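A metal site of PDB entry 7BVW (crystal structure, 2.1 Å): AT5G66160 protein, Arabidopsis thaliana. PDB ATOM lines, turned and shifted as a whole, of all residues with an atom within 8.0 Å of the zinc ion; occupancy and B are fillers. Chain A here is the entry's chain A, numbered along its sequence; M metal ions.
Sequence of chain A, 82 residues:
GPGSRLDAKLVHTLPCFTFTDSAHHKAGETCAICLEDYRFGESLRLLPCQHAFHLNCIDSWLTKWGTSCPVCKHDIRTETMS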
ATOM      1  N   LEU A  47     -16.944   4.188   1.037  1.00  0.00           N
ATOM      2  CA  LEU A  47     -17.941   3.411   0.320  1.00  0.00           C
ATOM      3  C   LEU A  47     -17.644   1.927   0.439  1.00  0.00           C
ATOM      4  O   LEU A  47     -16.495   1.538   0.645  1.00  0.00           O
ATOM      5  CB  LEU A  47     -17.988   3.833  -1.152  1.00  0.00           C
ATOM      6  CG  LEU A  47     -18.419   5.280  -1.452  1.00  0.00           C
ATOM      7  CD1 LEU A  47     -18.640   5.471  -2.949  1.00  0.00           C
ATOM      8  CD2 LEU A  47     -19.672   5.652  -0.666  1.00  0.00           C
ATOM      9  N   PRO A  48     -18.655   1.063   0.304  1.00  0.00           N
ATOM     10  CA  PRO A  48     -18.413  -0.380   0.480  1.00  0.00           C
ATOM     11  C   PRO A  48     -17.437  -0.970  -0.526  1.00  0.00           C
ATOM     12  O   PRO A  48     -16.862  -2.028  -0.253  1.00  0.00           O
ATOM     13  CB  PRO A  48     -19.807  -0.986   0.334  1.00  0.00           C
ATOM     14  CG  PRO A  48     -20.594   0.022  -0.426  1.00  0.00           C
ATOM     15  CD  PRO A  48     -20.071   1.357   0.033  1.00  0.00           C
ATOM     16  N   CYS A  49     -17.229  -0.318  -1.669  1.00  0.00           N
ATOM     17  CA  CYS A  49     -16.274  -0.789  -2.661  1.00  0.00           C
ATOM     18  C   CYS A  49     -14.837  -0.470  -2.288  1.00  0.00           C
ATOM     19  O   CYS A  49     -13.934  -0.776  -3.084  1.00  0.00           O
ATOM     20  CB  CYS A  49     -16.602  -0.172  -4.027  1.00  0.00           C
ATOM     21  SG  CYS A  49     -16.782   1.623  -3.967  1.00  0.00           S
ATOM     22  N   GLN A  50     -14.612   0.134  -1.111  1.00  0.00           N
ATOM     23  CA  GLN A  50     -13.300   0.434  -0.525  1.00  0.00           C
ATOM     24  C   GLN A  50     -12.660   1.693  -1.091  1.00  0.00           C
ATOM     25  O   GLN A  50     -11.435   1.859  -0.978  1.00  0.00           O
ATOM     26  CB  GLN A  50     -12.317  -0.742  -0.647  1.00  0.00           C
ATOM     27  CG  GLN A  50     -12.805  -2.041  -0.015  1.00  0.00           C
ATOM     28  CD  GLN A  50     -13.182  -1.873   1.436  1.00  0.00           C
ATOM     29  OE1 GLN A  50     -12.306  -1.746   2.297  1.00  0.00           O
ATOM     30  NE2 GLN A  50     -14.470  -1.871   1.722  1.00  0.00           N
ATOM     31  N   HIS A  51     -13.433   2.590  -1.688  1.00  0.00           N
ATOM     32  CA  HIS A  51     -12.936   3.887  -2.119  1.00  0.00           C
ATOM     33  C   HIS A  51     -13.420   4.967  -1.169  1.00  0.00           C
ATOM     34  O   HIS A  51     -14.589   4.983  -0.775  1.00  0.00           O
ATOM     35  CB  HIS A  51     -13.376   4.214  -3.542  1.00  0.00           C
ATOM     36  CG  HIS A  51     -12.831   3.287  -4.579  1.00  0.00           C
ATOM     37  ND1 HIS A  51     -13.633   2.451  -5.330  1.00  0.00           N
ATOM     38  CD2 HIS A  51     -11.564   3.053  -4.987  1.00  0.00           C
ATOM     39  CE1 HIS A  51     -12.882   1.744  -6.155  1.00  0.00           C
ATOM     40  NE2 HIS A  51     -11.613   2.088  -5.965  1.00  0.00           N
ATOM     41  N   ALA A  52     -12.523   5.882  -0.802  1.00  0.00           N
ATOM     42  CA  ALA A  52     -12.831   6.955   0.137  1.00  0.00           C
ATOM     43  C   ALA A  52     -12.772   8.301  -0.561  1.00  0.00           C
ATOM     44  O   ALA A  52     -12.082   8.484  -1.565  1.00  0.00           O
ATOM     45  CB  ALA A  52     -11.860   6.940   1.325  1.00  0.00           C
ATOM     46  N   PHE A  53     -13.533   9.249  -0.011  1.00  0.00           N
ATOM     47  CA  PHE A  53     -13.624  10.582  -0.578  1.00  0.00           C
ATOM     48  C   PHE A  53     -13.771  11.593   0.541  1.00  0.00           C
ATOM     49  O   PHE A  53     -14.021  11.238   1.697  1.00  0.00           O
ATOM     50  CB  PHE A  53     -14.814  10.724  -1.539  1.00  0.00           C
ATOM     51  CG  PHE A  53     -14.893   9.646  -2.584  1.00  0.00           C
ATOM     52  CD1 PHE A  53     -15.537   8.445  -2.315  1.00  0.00           C
ATOM     53  CD2 PHE A  53     -14.357   9.856  -3.841  1.00  0.00           C
ATOM     54  CE1 PHE A  53     -15.607   7.462  -3.287  1.00  0.00           C
ATOM     55  CE2 PHE A  53     -14.437   8.864  -4.809  1.00  0.00           C
ATOM     56  CZ  PHE A  53     -15.063   7.669  -4.528  1.00  0.00           C
ATOM     57  N   SER A  68     -23.922   5.448  -7.537  1.00  0.00           N
ATOM     58  CA  SER A  68     -22.828   4.508  -7.579  1.00  0.00           C
ATOM     59  C   SER A  68     -21.538   5.226  -7.215  1.00  0.00           C
ATOM     60  O   SER A  68     -21.486   6.460  -7.165  1.00  0.00           O
ATOM     61  CB  SER A  68     -22.710   3.842  -8.960  1.00  0.00           C
ATOM     62  OG  SER A  68     -22.288   4.776  -9.942  1.00  0.00           O
ATOM     63  N   CYS A  69     -20.491   4.452  -6.987  1.00  0.00           N
ATOM     64  CA  CYS A  69     -19.182   5.024  -6.718  1.00  0.00           C
ATOM     65  C   CYS A  69     -18.660   5.730  -7.965  1.00  0.00           C
ATOM     66  O   CYS A  69     -18.639   5.134  -9.048  1.00  0.00           O
ATOM     67  CB  CYS A  69     -18.199   3.934  -6.283  1.00  0.00           C
ATOM     68  SG  CYS A  69     -16.485   4.488  -6.182  1.00  0.00           S
ATOM     69  N   PRO A  70     -18.242   7.008  -7.863  1.00  0.00           N
ATOM     70  CA  PRO A  70     -17.751   7.715  -9.058  1.00  0.00           C
ATOM     71  C   PRO A  70     -16.404   7.228  -9.571  1.00  0.00           C
ATOM     72  O   PRO A  70     -15.944   7.733 -10.602  1.00  0.00           O
ATOM     73  CB  PRO A  70     -17.662   9.172  -8.569  1.00  0.00           C
ATOM     74  CG  PRO A  70     -17.504   9.066  -7.095  1.00  0.00           C
ATOM     75  CD  PRO A  70     -18.300   7.863  -6.680  1.00  0.00           C
ATOM     76  N   VAL A  71     -15.764   6.275  -8.909  1.00  0.00           N
ATOM     77  CA  VAL A  71     -14.469   5.761  -9.357  1.00  0.00           C
ATOM     78  C   VAL A  71     -14.652   4.426 -10.073  1.00  0.00           C
ATOM     79  O   VAL A  71     -14.237   4.261 -11.221  1.00  0.00           O
ATOM     80  CB  VAL A  71     -13.488   5.628  -8.185  1.00  0.00           C
ATOM     81  CG1 VAL A  71     -12.188   4.976  -8.662  1.00  0.00           C
ATOM     82  CG2 VAL A  71     -13.214   6.986  -7.571  1.00  0.00           C
ATOM     83  N   CYS A  72     -15.284   3.465  -9.396  1.00  0.00           N
ATOM     84  CA  CYS A  72     -15.433   2.118  -9.924  1.00  0.00           C
ATOM     85  C   CYS A  72     -16.861   1.786 -10.334  1.00  0.00           C
ATOM     86  O   CYS A  72     -17.109   0.672 -10.809  1.00  0.00           O
ATOM     87  CB  CYS A  72     -14.935   1.087  -8.901  1.00  0.00           C
ATOM     88  SG  CYS A  72     -16.025   0.852  -7.486  1.00  0.00           S
ATOM     89  N   LYS A  73     -17.798   2.717 -10.160  1.00  0.00           N
ATOM     90  CA  LYS A  73     -19.194   2.573 -10.589  1.00  0.00           C
ATOM     91  C   LYS A  73     -19.919   1.426  -9.897  1.00  0.00           C
ATOM     92  O   LYS A  73     -20.914   0.913 -10.410  1.00  0.00           O
ATOM     93  CB  LYS A  73     -19.294   2.427 -12.114  1.00  0.00           C
ATOM     94  CG  LYS A  73     -18.942   3.701 -12.873  1.00  0.00           C
ATOM     95  N   HIS A  74     -19.443   1.021  -8.721  1.00  0.00           N
ATOM     96  CA  HIS A  74     -20.165   0.051  -7.902  1.00  0.00           C
ATOM     97  C   HIS A  74     -21.516   0.624  -7.496  1.00  0.00           C
ATOM     98  O   HIS A  74     -21.582   1.651  -6.821  1.00  0.00           O
ATOM     99  CB  HIS A  74     -19.344  -0.321  -6.673  1.00  0.00           C
ATOM    100  CG  HIS A  74     -20.141  -0.987  -5.595  1.00  0.00           C
ATOM    101  ND1 HIS A  74     -20.365  -2.349  -5.567  1.00  0.00           N
ATOM    102  CD2 HIS A  74     -20.760  -0.476  -4.508  1.00  0.00           C
ATOM    103  CE1 HIS A  74     -21.092  -2.644  -4.498  1.00  0.00           C
ATOM    104  NE2 HIS A  74     -21.343  -1.531  -3.842  1.00  0.00           N
ATOM    105  N   ASP A  75     -22.584  -0.046  -7.909  1.00  0.00           N
ATOM    106  CA  ASP A  75     -23.931   0.481  -7.704  1.00  0.00           C
ATOM    107  C   ASP A  75     -24.407   0.230  -6.283  1.00  0.00           C
ATOM    108  O   ASP A  75     -24.218  -0.852  -5.722  1.00  0.00           O
ATOM    109  CB  ASP A  75     -24.900  -0.153  -8.694  1.00  0.00           C
ATOM    110  CG  ASP A  75     -24.606   0.247 -10.126  1.00  0.00           C
ATOM    111  OD1 ASP A  75     -24.237   1.416 -10.345  1.00  0.00           O
ATOM    112  OD2 ASP A  75     -24.721  -0.620 -11.015  1.00  0.00           O
HETATM  113 ZN    ZN M   1     -15.605   2.378  -5.768  1.00  0.00          ZN
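The side-chain sulfur (SG) of Cys 69 sits close to the backbone NH (N) of Val 71, 3.3 Å away. The backbone NH (N) of Cys 69 is in hydrogen-bond range of the backbone carbonyl oxygen (O) of His 74, 3.0 Å away. The side-chain sulfur (SG) of Cys 72 sits close to the backbone NH (N) of His 74 (3.6 Å).
The zinc ion is bound by ND1 of His 51 (2.0 Å), SG of Cys 49 (2.3 Å), SG of Cys 69 (2.3 Å) and SG of Cys 72 (2.3 Å).
Of the 15 residues printed, 4 come within 4 Å of the zinc ion. Along chain A the residues within 4 Å of the zinc ion span positions 49 to 72. The nearest printed residue that does not touch the zinc ion is Val 71 (4.6 Å).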
